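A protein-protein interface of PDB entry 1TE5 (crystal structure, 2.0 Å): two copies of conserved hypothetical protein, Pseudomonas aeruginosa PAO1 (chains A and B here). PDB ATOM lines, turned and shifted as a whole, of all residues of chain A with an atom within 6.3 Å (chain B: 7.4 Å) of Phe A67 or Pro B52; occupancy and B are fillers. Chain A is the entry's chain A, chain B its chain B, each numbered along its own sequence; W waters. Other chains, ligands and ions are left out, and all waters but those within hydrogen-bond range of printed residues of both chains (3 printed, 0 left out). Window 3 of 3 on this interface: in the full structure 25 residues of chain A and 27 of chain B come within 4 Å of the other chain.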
ATOM      1  N   ILE A  15      15.544   4.750 -23.623  1.00  0.00           N
ATOM      2  CA  ILE A  15      14.235   5.399 -23.610  1.00  0.00           C
ATOM      3  C   ILE A  15      14.367   6.676 -22.773  1.00  0.00           C
ATOM      4  O   ILE A  15      14.517   6.604 -21.551  1.00  0.00           O
ATOM      5  CB  ILE A  15      13.151   4.524 -22.947  1.00  0.00           C
ATOM      6  CG1 ILE A  15      13.105   3.147 -23.581  1.00  0.00           C
ATOM      7  CG2 ILE A  15      11.792   5.168 -23.109  1.00  0.00           C
ATOM      8  CD1 ILE A  15      11.995   2.292 -23.042  1.00  0.00           C
ATOM      9  N   PHE A  40      10.559  -0.291 -15.102  1.00  0.00           N
ATOM     10  CA  PHE A  40      11.323  -0.978 -16.129  1.00  0.00           C
ATOM     11  C   PHE A  40      12.284  -1.972 -15.495  1.00  0.00           C
ATOM     12  O   PHE A  40      12.561  -1.897 -14.299  1.00  0.00           O
ATOM     13  CB  PHE A  40      12.041   0.008 -17.062  1.00  0.00           C
ATOM     14  CG  PHE A  40      13.017   0.910 -16.375  1.00  0.00           C
ATOM     15  CD1 PHE A  40      14.377   0.592 -16.343  1.00  0.00           C
ATOM     16  CD2 PHE A  40      12.587   2.099 -15.791  1.00  0.00           C
ATOM     17  CE1 PHE A  40      15.307   1.450 -15.737  1.00  0.00           C
ATOM     18  CE2 PHE A  40      13.497   2.965 -15.182  1.00  0.00           C
ATOM     19  CZ  PHE A  40      14.863   2.640 -15.156  1.00  0.00           C
ATOM     20  N   GLU A  42      15.961  -4.338 -15.244  1.00  0.00           N
ATOM     21  CA  GLU A  42      17.404  -4.379 -15.411  1.00  0.00           C
ATOM     22  C   GLU A  42      17.831  -5.775 -14.969  1.00  0.00           C
ATOM     23  O   GLU A  42      18.388  -6.006 -13.892  1.00  0.00           O
ATOM     24  CB  GLU A  42      18.036  -3.361 -14.468  1.00  0.00           C
ATOM     25  CG  GLU A  42      19.245  -2.638 -15.014  1.00  0.00           C
ATOM     26  CD  GLU A  42      19.522  -1.342 -14.263  1.00  0.00           C
ATOM     27  OE1 GLU A  42      18.826  -0.336 -14.533  1.00  0.00           O
ATOM     28  OE2 GLU A  42      20.433  -1.332 -13.406  1.00  0.00           O
ATOM     29  N   ARG A  47      12.947  -1.171 -11.617  1.00  0.00           N
ATOM     30  CA  ARG A  47      13.050   0.196 -11.112  1.00  0.00           C
ATOM     31  C   ARG A  47      11.686   0.862 -11.246  1.00  0.00           C
ATOM     32  O   ARG A  47      11.016   0.711 -12.258  1.00  0.00           O
ATOM     33  CB  ARG A  47      14.094   0.994 -11.888  1.00  0.00           C
ATOM     34  CG  ARG A  47      15.508   0.490 -11.721  1.00  0.00           C
ATOM     35  CD  ARG A  47      16.489   1.474 -12.300  1.00  0.00           C
ATOM     36  NE  ARG A  47      17.862   0.981 -12.282  1.00  0.00           N
ATOM     37  CZ  ARG A  47      18.726   1.177 -11.290  1.00  0.00           C
ATOM     38  NH1 ARG A  47      19.952   0.686 -11.380  1.00  0.00           N
ATOM     39  NH2 ARG A  47      18.364   1.860 -10.208  1.00  0.00           N
ATOM     40  N   PHE A  49       9.550   4.592 -10.724  1.00  0.00           N
ATOM     41  CA  PHE A  49       9.517   6.029 -10.492  1.00  0.00           C
ATOM     42  C   PHE A  49       8.061   6.396 -10.720  1.00  0.00           C
ATOM     43  O   PHE A  49       7.515   6.135 -11.795  1.00  0.00           O
ATOM     44  CB  PHE A  49      10.383   6.774 -11.509  1.00  0.00           C
ATOM     45  CG  PHE A  49      11.813   6.306 -11.570  1.00  0.00           C
ATOM     46  CD1 PHE A  49      12.204   5.324 -12.482  1.00  0.00           C
ATOM     47  CD2 PHE A  49      12.780   6.860 -10.729  1.00  0.00           C
ATOM     48  CE1 PHE A  49      13.531   4.901 -12.555  1.00  0.00           C
ATOM     49  CE2 PHE A  49      14.114   6.440 -10.796  1.00  0.00           C
ATOM     50  CZ  PHE A  49      14.484   5.455 -11.715  1.00  0.00           C
ATOM     51  N   ARG A  62      12.119  14.535 -11.856  1.00  0.00           N
ATOM     52  CA  ARG A  62      13.439  14.884 -12.356  1.00  0.00           C
ATOM     53  C   ARG A  62      14.297  13.623 -12.409  1.00  0.00           C
ATOM     54  O   ARG A  62      15.191  13.500 -13.250  1.00  0.00           O
ATOM     55  CB  ARG A  62      14.106  15.913 -11.440  1.00  0.00           C
ATOM     56  CG  ARG A  62      13.666  17.345 -11.667  1.00  0.00           C
ATOM     57  CD  ARG A  62      14.601  18.319 -10.950  1.00  0.00           C
ATOM     58  NE  ARG A  62      14.268  18.502  -9.542  1.00  0.00           N
ATOM     59  CZ  ARG A  62      13.195  19.163  -9.116  1.00  0.00           C
ATOM     60  NH1 ARG A  62      12.960  19.295  -7.817  1.00  0.00           N
ATOM     61  NH2 ARG A  62      12.356  19.696  -9.994  1.00  0.00           N
ATOM     62  N   LEU A  63      14.048  12.711 -11.474  1.00  0.00           N
ATOM     63  CA  LEU A  63      14.783  11.462 -11.402  1.00  0.00           C
ATOM     64  C   LEU A  63      14.629  10.588 -12.651  1.00  0.00           C
ATOM     65  O   LEU A  63      15.621  10.065 -13.157  1.00  0.00           O
ATOM     66  CB  LEU A  63      14.393  10.696 -10.138  1.00  0.00           C
ATOM     67  CG  LEU A  63      15.419  10.640  -9.001  1.00  0.00           C
ATOM     68  CD1 LEU A  63      16.559   9.729  -9.401  1.00  0.00           C
ATOM     69  CD2 LEU A  63      15.932  12.031  -8.657  1.00  0.00           C
ATOM     70  N   VAL A  64      13.403  10.409 -13.145  1.00  0.00           N
ATOM     71  CA  VAL A  64      13.187   9.598 -14.353  1.00  0.00           C
ATOM     72  C   VAL A  64      13.914  10.175 -15.553  1.00  0.00           C
ATOM     73  O   VAL A  64      14.385   9.432 -16.419  1.00  0.00           O
ATOM     74  CB  VAL A  64      11.714   9.512 -14.781  1.00  0.00           C
ATOM     75  CG1 VAL A  64      11.055   8.320 -14.159  1.00  0.00           C
ATOM     76  CG2 VAL A  64      10.991  10.796 -14.463  1.00  0.00           C
ATOM     77  N   GLN A  65      13.935  11.502 -15.630  1.00  0.00           N
ATOM     78  CA  GLN A  65      14.585  12.198 -16.729  1.00  0.00           C
ATOM     79  C   GLN A  65      16.105  12.186 -16.683  1.00  0.00           C
ATOM     80  O   GLN A  65      16.741  12.180 -17.738  1.00  0.00           O
ATOM     81  CB  GLN A  65      14.083  13.634 -16.812  1.00  0.00           C
ATOM     82  CG  GLN A  65      12.596  13.735 -17.039  1.00  0.00           C
ATOM     83  CD  GLN A  65      12.162  15.134 -17.405  1.00  0.00           C
ATOM     84  OE1 GLN A  65      12.512  15.656 -18.473  1.00  0.00           O
ATOM     85  NE2 GLN A  65      11.418  15.764 -16.509  1.00  0.00           N
ATOM     86  N   ARG A  66      16.694  12.204 -15.486  1.00  0.00           N
ATOM     87  CA  ARG A  66      18.154  12.199 -15.370  1.00  0.00           C
ATOM     88  C   ARG A  66      18.819  10.814 -15.400  1.00  0.00           C
ATOM     89  O   ARG A  66      20.029  10.689 -15.618  1.00  0.00           O
ATOM     90  CB  ARG A  66      18.612  13.023 -14.154  1.00  0.00           C
ATOM     91  CG  ARG A  66      18.040  12.604 -12.818  1.00  0.00           C
ATOM     92  CD  ARG A  66      18.371  13.623 -11.717  1.00  0.00           C
ATOM     93  NE  ARG A  66      19.787  13.626 -11.343  1.00  0.00           N
ATOM     94  CZ  ARG A  66      20.249  13.928 -10.129  1.00  0.00           C
ATOM     95  NH1 ARG A  66      21.555  13.901  -9.886  1.00  0.00           N
ATOM     96  NH2 ARG A  66      19.411  14.254  -9.149  1.00  0.00           N
ATOM     97  N   PHE A  67      18.013   9.777 -15.209  1.00  0.00           N
ATOM     98  CA  PHE A  67      18.502   8.403 -15.198  1.00  0.00           C
ATOM     99  C   PHE A  67      18.651   7.823 -16.604  1.00  0.00           C
ATOM    100  O   PHE A  67      17.696   7.802 -17.374  1.00  0.00           O
ATOM    101  CB  PHE A  67      17.539   7.521 -14.381  1.00  0.00           C
ATOM    102  CG  PHE A  67      17.990   6.086 -14.239  1.00  0.00           C
ATOM    103  CD1 PHE A  67      18.786   5.694 -13.173  1.00  0.00           C
ATOM    104  CD2 PHE A  67      17.631   5.131 -15.181  1.00  0.00           C
ATOM    105  CE1 PHE A  67      19.221   4.373 -13.048  1.00  0.00           C
ATOM    106  CE2 PHE A  67      18.060   3.812 -15.063  1.00  0.00           C
ATOM    107  CZ  PHE A  67      18.858   3.435 -13.996  1.00  0.00           C
ATOM    108  N   PRO A  68      19.868   7.388 -16.976  1.00  0.00           N
ATOM    109  CA  PRO A  68      20.031   6.808 -18.315  1.00  0.00           C
ATOM    110  C   PRO A  68      19.353   5.439 -18.297  1.00  0.00           C
ATOM    111  O   PRO A  68      19.891   4.487 -17.749  1.00  0.00           O
ATOM    112  CB  PRO A  68      21.552   6.676 -18.449  1.00  0.00           C
ATOM    113  CG  PRO A  68      22.072   7.757 -17.561  1.00  0.00           C
ATOM    114  CD  PRO A  68      21.177   7.627 -16.353  1.00  0.00           C
ATOM    115  N   ILE A  69      18.121   5.392 -18.785  1.00  0.00           N
ATOM    116  CA  ILE A  69      17.337   4.168 -18.828  1.00  0.00           C
ATOM    117  C   ILE A  69      17.691   3.301 -20.037  1.00  0.00           C
ATOM    118  O   ILE A  69      17.897   3.807 -21.144  1.00  0.00           O
ATOM    119  CB  ILE A  69      15.823   4.484 -18.869  1.00  0.00           C
ATOM    120  CG1 ILE A  69      15.413   5.328 -17.659  1.00  0.00           C
ATOM    121  CG2 ILE A  69      15.017   3.196 -18.923  1.00  0.00           C
ATOM    122  CD1 ILE A  69      13.941   5.680 -17.624  1.00  0.00           C
ATOM    123  N   LYS A  70      17.754   1.993 -19.818  1.00  0.00           N
ATOM    124  CA  LYS A  70      18.069   1.047 -20.880  1.00  0.00           C
ATOM    125  C   LYS A  70      17.564  -0.338 -20.469  1.00  0.00           C
ATOM    126  O   LYS A  70      18.223  -1.040 -19.700  1.00  0.00           O
ATOM    127  CB  LYS A  70      19.577   1.021 -21.117  1.00  0.00           C
ATOM    128  CG  LYS A  70      19.992   0.359 -22.413  1.00  0.00           C
ATOM    129  CD  LYS A  70      21.493   0.113 -22.470  1.00  0.00           C
ATOM    130  CE  LYS A  70      22.297   1.404 -22.579  1.00  0.00           C
ATOM    131  NZ  LYS A  70      22.169   2.053 -23.917  1.00  0.00           N
ATOM    132  N   ARG B  33      31.956   3.157  -8.075  1.00  0.00           N
ATOM    133  CA  ARG B  33      31.150   3.613  -6.952  1.00  0.00           C
ATOM    134  C   ARG B  33      30.534   2.427  -6.231  1.00  0.00           C
ATOM    135  O   ARG B  33      30.102   1.461  -6.868  1.00  0.00           O
ATOM    136  CB  ARG B  33      30.023   4.536  -7.430  1.00  0.00           C
ATOM    137  CG  ARG B  33      29.085   4.993  -6.308  1.00  0.00           C
ATOM    138  CD  ARG B  33      27.928   5.843  -6.828  1.00  0.00           C
ATOM    139  NE  ARG B  33      28.376   7.061  -7.510  1.00  0.00           N
ATOM    140  CZ  ARG B  33      28.979   8.089  -6.913  1.00  0.00           C
ATOM    141  NH1 ARG B  33      29.341   9.145  -7.633  1.00  0.00           N
ATOM    142  NH2 ARG B  33      29.231   8.065  -5.605  1.00  0.00           N
ATOM    143  N   TRP B  36      24.312   1.633  -3.454  1.00  0.00           N
ATOM    144  CA  TRP B  36      23.502   2.186  -2.386  1.00  0.00           C
ATOM    145  C   TRP B  36      22.041   1.965  -2.733  1.00  0.00           C
ATOM    146  O   TRP B  36      21.689   1.714  -3.887  1.00  0.00           O
ATOM    147  CB  TRP B  36      23.800   3.679  -2.182  1.00  0.00           C
ATOM    148  CG  TRP B  36      23.629   4.530  -3.418  1.00  0.00           C
ATOM    149  CD1 TRP B  36      24.580   4.809  -4.357  1.00  0.00           C
ATOM    150  CD2 TRP B  36      22.433   5.201  -3.848  1.00  0.00           C
ATOM    151  NE1 TRP B  36      24.052   5.609  -5.348  1.00  0.00           N
ATOM    152  CE2 TRP B  36      22.737   5.862  -5.059  1.00  0.00           C
ATOM    153  CE3 TRP B  36      21.134   5.306  -3.327  1.00  0.00           C
ATOM    154  CZ2 TRP B  36      21.787   6.616  -5.759  1.00  0.00           C
ATOM    155  CZ3 TRP B  36      20.191   6.058  -4.025  1.00  0.00           C
ATOM    156  CH2 TRP B  36      20.524   6.701  -5.227  1.00  0.00           C
ATOM    157  N   PHE B  49      15.041   3.950  -4.431  1.00  0.00           N
ATOM    158  CA  PHE B  49      16.056   4.492  -5.331  1.00  0.00           C
ATOM    159  C   PHE B  49      17.350   3.762  -5.095  1.00  0.00           C
ATOM    160  O   PHE B  49      17.844   3.696  -3.975  1.00  0.00           O
ATOM    161  CB  PHE B  49      16.293   5.983  -5.076  1.00  0.00           C
ATOM    162  CG  PHE B  49      15.088   6.822  -5.301  1.00  0.00           C
ATOM    163  CD1 PHE B  49      14.433   7.414  -4.225  1.00  0.00           C
ATOM    164  CD2 PHE B  49      14.575   6.997  -6.591  1.00  0.00           C
ATOM    165  CE1 PHE B  49      13.266   8.176  -4.424  1.00  0.00           C
ATOM    166  CE2 PHE B  49      13.409   7.756  -6.810  1.00  0.00           C
ATOM    167  CZ  PHE B  49      12.751   8.348  -5.723  1.00  0.00           C
ATOM    168  N   GLN B  50      17.916   3.254  -6.173  1.00  0.00           N
ATOM    169  CA  GLN B  50      19.167   2.532  -6.107  1.00  0.00           C
ATOM    170  C   GLN B  50      20.146   3.169  -7.084  1.00  0.00           C
ATOM    171  O   GLN B  50      19.735   3.790  -8.062  1.00  0.00           O
ATOM    172  CB  GLN B  50      18.913   1.042  -6.378  1.00  0.00           C
ATOM    173  CG  GLN B  50      18.174   0.370  -5.212  1.00  0.00           C
ATOM    174  CD  GLN B  50      17.217  -0.710  -5.647  1.00  0.00           C
ATOM    175  OE1 GLN B  50      17.187  -1.788  -5.057  1.00  0.00           O
ATOM    176  NE2 GLN B  50      16.395  -0.416  -6.660  1.00  0.00           N
ATOM    177  N   ASP B  51      21.435   3.077  -6.776  1.00  0.00           N
ATOM    178  CA  ASP B  51      22.461   3.681  -7.616  1.00  0.00           C
ATOM    179  C   ASP B  51      22.278   3.471  -9.113  1.00  0.00           C
ATOM    180  O   ASP B  51      21.913   2.385  -9.566  1.00  0.00           O
ATOM    181  CB  ASP B  51      23.875   3.262  -7.177  1.00  0.00           C
ATOM    182  CG  ASP B  51      24.221   1.833  -7.550  1.00  0.00           C
ATOM    183  OD1 ASP B  51      23.739   0.897  -6.869  1.00  0.00           O
ATOM    184  OD2 ASP B  51      25.010   1.653  -8.509  1.00  0.00           O
ATOM    185  N   PRO B  52      22.442   4.549  -9.894  1.00  0.00           N
ATOM    186  CA  PRO B  52      22.307   4.492 -11.350  1.00  0.00           C
ATOM    187  C   PRO B  52      23.396   3.598 -11.940  1.00  0.00           C
ATOM    188  O   PRO B  52      24.475   3.448 -11.356  1.00  0.00           O
ATOM    189  CB  PRO B  52      22.514   5.952 -11.765  1.00  0.00           C
ATOM    190  CG  PRO B  52      22.010   6.724 -10.572  1.00  0.00           C
ATOM    191  CD  PRO B  52      22.619   5.941  -9.439  1.00  0.00           C
ATOM    192  N   LEU B  53      23.102   2.999 -13.087  1.00  0.00           N
ATOM    193  CA  LEU B  53      24.070   2.139 -13.755  1.00  0.00           C
ATOM    194  C   LEU B  53      24.901   2.984 -14.735  1.00  0.00           C
ATOM    195  O   LEU B  53      24.967   2.695 -15.936  1.00  0.00           O
ATOM    196  CB  LEU B  53      23.354   0.987 -14.482  1.00  0.00           C
ATOM    197  CG  LEU B  53      24.055  -0.382 -14.563  1.00  0.00           C
ATOM    198  CD1 LEU B  53      23.088  -1.413 -15.129  1.00  0.00           C
ATOM    199  CD2 LEU B  53      25.341  -0.324 -15.394  1.00  0.00           C
ATOM    200  N   ALA B  54      25.470   4.073 -14.223  1.00  0.00           N
ATOM    201  CA  ALA B  54      26.305   4.970 -15.021  1.00  0.00           C
ATOM    202  C   ALA B  54      27.739   4.954 -14.467  1.00  0.00           C
ATOM    203  O   ALA B  54      28.547   4.105 -14.865  1.00  0.00           O
ATOM    204  CB  ALA B  54      25.723   6.400 -15.021  1.00  0.00           C
ATOM    205  N   SER B  55      28.029   5.856 -13.524  1.00  0.00           N
ATOM    206  CA  SER B  55      29.355   5.988 -12.894  1.00  0.00           C
ATOM    207  C   SER B  55      30.522   6.210 -13.874  1.00  0.00           C
ATOM    208  O   SER B  55      31.678   6.367 -13.462  1.00  0.00           O
ATOM    209  CB  SER B  55      29.641   4.826 -11.925  1.00  0.00           C
ATOM    210  OG  SER B  55      29.107   5.091 -10.629  1.00  0.00           O
ATOM    211  N   GLN B  65      26.735  14.781  -6.100  1.00  0.00           N
ATOM    212  CA  GLN B  65      25.361  14.750  -6.588  1.00  0.00           C
ATOM    213  C   GLN B  65      24.397  14.625  -5.412  1.00  0.00           C
ATOM    214  O   GLN B  65      24.583  13.775  -4.548  1.00  0.00           O
ATOM    215  CB  GLN B  65      25.186  13.587  -7.567  1.00  0.00           C
ATOM    216  CG  GLN B  65      26.135  13.660  -8.754  1.00  0.00           C
ATOM    217  CD  GLN B  65      26.122  12.412  -9.613  1.00  0.00           C
ATOM    218  OE1 GLN B  65      25.381  12.333 -10.595  1.00  0.00           O
ATOM    219  NE2 GLN B  65      26.959  11.437  -9.263  1.00  0.00           N
ATOM    220  N   PHE B  67      20.568  14.167  -3.488  1.00  0.00           N
ATOM    221  CA  PHE B  67      19.342  13.360  -3.537  1.00  0.00           C
ATOM    222  C   PHE B  67      18.419  13.679  -2.375  1.00  0.00           C
ATOM    223  O   PHE B  67      18.468  13.038  -1.329  1.00  0.00           O
ATOM    224  CB  PHE B  67      19.663  11.862  -3.566  1.00  0.00           C
ATOM    225  CG  PHE B  67      20.334  11.430  -4.834  1.00  0.00           C
ATOM    226  CD1 PHE B  67      19.582  11.099  -5.957  1.00  0.00           C
ATOM    227  CD2 PHE B  67      21.725  11.432  -4.938  1.00  0.00           C
ATOM    228  CE1 PHE B  67      20.211  10.781  -7.177  1.00  0.00           C
ATOM    229  CE2 PHE B  67      22.364  11.116  -6.150  1.00  0.00           C
ATOM    230  CZ  PHE B  67      21.602  10.791  -7.270  1.00  0.00           C
ATOM    231  N   ASN B  82      28.607  -1.286  -6.718  1.00  0.00           N
ATOM    232  CA  ASN B  82      27.984  -0.689  -7.895  1.00  0.00           C
ATOM    233  C   ASN B  82      26.973  -1.692  -8.450  1.00  0.00           C
ATOM    234  O   ASN B  82      27.277  -2.879  -8.566  1.00  0.00           O
ATOM    235  CB  ASN B  82      29.055  -0.360  -8.941  1.00  0.00           C
ATOM    236  CG  ASN B  82      28.475  -0.104 -10.326  1.00  0.00           C
ATOM    237  OD1 ASN B  82      29.003  -0.602 -11.327  1.00  0.00           O
ATOM    238  ND2 ASN B  82      27.397   0.676 -10.398  1.00  0.00           N
ATOM    239  N   VAL B  83      25.752  -1.233  -8.702  1.00  0.00           N
ATOM    240  CA  VAL B  83      24.704  -2.110  -9.224  1.00  0.00           C
ATOM    241  C   VAL B  83      25.183  -2.922 -10.445  1.00  0.00           C
ATOM    242  O   VAL B  83      24.588  -3.935 -10.809  1.00  0.00           O
ATOM    243  CB  VAL B  83      23.409  -1.301  -9.553  1.00  0.00           C
ATOM    244  CG1 VAL B  83      23.340  -0.929 -11.033  1.00  0.00           C
ATOM    245  CG2 VAL B  83      22.181  -2.073  -9.122  1.00  0.00           C
ATOM    246  N   GLY B  84      26.245  -2.453 -11.087  1.00  0.00           N
ATOM    247  CA  GLY B  84      26.775  -3.160 -12.234  1.00  0.00           C
ATOM    248  C   GLY B  84      27.563  -4.378 -11.795  1.00  0.00           C
ATOM    249  O   GLY B  84      27.783  -5.302 -12.583  1.00  0.00           O
ATOM    250  N   LEU B  88      20.944  -5.326 -10.061  1.00  0.00           N
ATOM    251  CA  LEU B  88      19.820  -4.682  -9.399  1.00  0.00           C
ATOM    252  C   LEU B  88      19.017  -5.606  -8.468  1.00  0.00           C
ATOM    253  O   LEU B  88      18.559  -5.175  -7.408  1.00  0.00           O
ATOM    254  CB  LEU B  88      18.894  -4.051 -10.441  1.00  0.00           C
ATOM    255  CG  LEU B  88      17.712  -3.231  -9.916  1.00  0.00           C
ATOM    256  CD1 LEU B  88      18.212  -2.013  -9.151  1.00  0.00           C
ATOM    257  CD2 LEU B  88      16.829  -2.806 -11.068  1.00  0.00           C
HETATM  258  O   HOH W   1      19.393  -7.604 -11.487  1.00  0.00           O
HETATM  259  O   HOH W   2      21.401  -3.959 -12.811  1.00  0.00           O
HETATM  260  O   HOH W   3      15.901   3.882  -8.809  1.00  0.00           O
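NH2 of Arg A47 lies within hydrogen-bond range of O of Gln B50 (3.2 Å).
NH1 of Arg A47 sits at hydrogen-bond distance from O of Asp B51 (3.2 Å).
The backbone carbonyl oxygen of Trp B36 sits at hydrogen-bond distance from the backbone NH of Asp B51, 3.2 Å away.
The side-chain carboxylate (OD2) of Asp B51 sits at hydrogen-bond distance from the backbone NH (N) of Val B83 (3.0 Å).
OE1 of Glu A42 is in salt-bridge range of NE of Arg A47, 2.8 Å away.
The backbone carbonyl oxygen of Phe A40 is in hydrogen-bond range of the backbone NH of Arg A47.
OD2 of Asp B51 lies within hydrogen-bond range of ND2 of Asn B82, 3.2 Å away.
Among the printed residues, pairs that only touch across the chains: Glu A42 with Leu B53 (3.2 Å), Phe A67 with Pro B52 (3.5 Å), Arg A47 with Leu B88 (3.6 Å), Glu A42 with Leu B88 (3.7 Å), Arg A47 with Val B83 (3.8 Å) and Glu A42 with Val B83 (3.8 Å).
Phe A67 touches just one residue of chain B: Pro B52.
Of the printed residues of chain A, Leu B88 touches Glu A42 (3.7 Å) and Arg A47 (3.6 Å).
Printed residues of chain A within 4 Å of Asp B51: Arg A47.
Of the printed residues of chain B, Arg A47 touches Gln B50, Asp B51, Val B83 and Leu B88.
Of the printed residues of chain A, Gln B50 touches Arg A47.
The nearest residue of chain B that does not touch Phe A67 is Leu B53 (4.1 Å).
The nearest printed residue of chain A that does not touch Leu B88 is Phe A40 (5.4 Å).
Of the 14 printed residues of chain A, 3 touch a printed residue of chain B.
Along chain A the printed residues that touch a printed residue of chain B span positions 42 to 67.
Of the 15 printed residues of chain B, 6 touch a printed residue of chain A.
Positions printed for both chains: 49, 65 and 67.
Water W2 lies within hydrogen-bond range of the side-chain carboxylate (OE2) of Glu A42 and the backbone NH (N) of Leu B88.
Water W1 bridges O of Glu A42 (3.1 Å) and N of Leu B88 (3.1 Å).
Water W3 bridges the backbone NH (N) of Gln B50 (3.4 Å) and the guanidinium group (NH2) of Arg A47 (3.5 Å).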
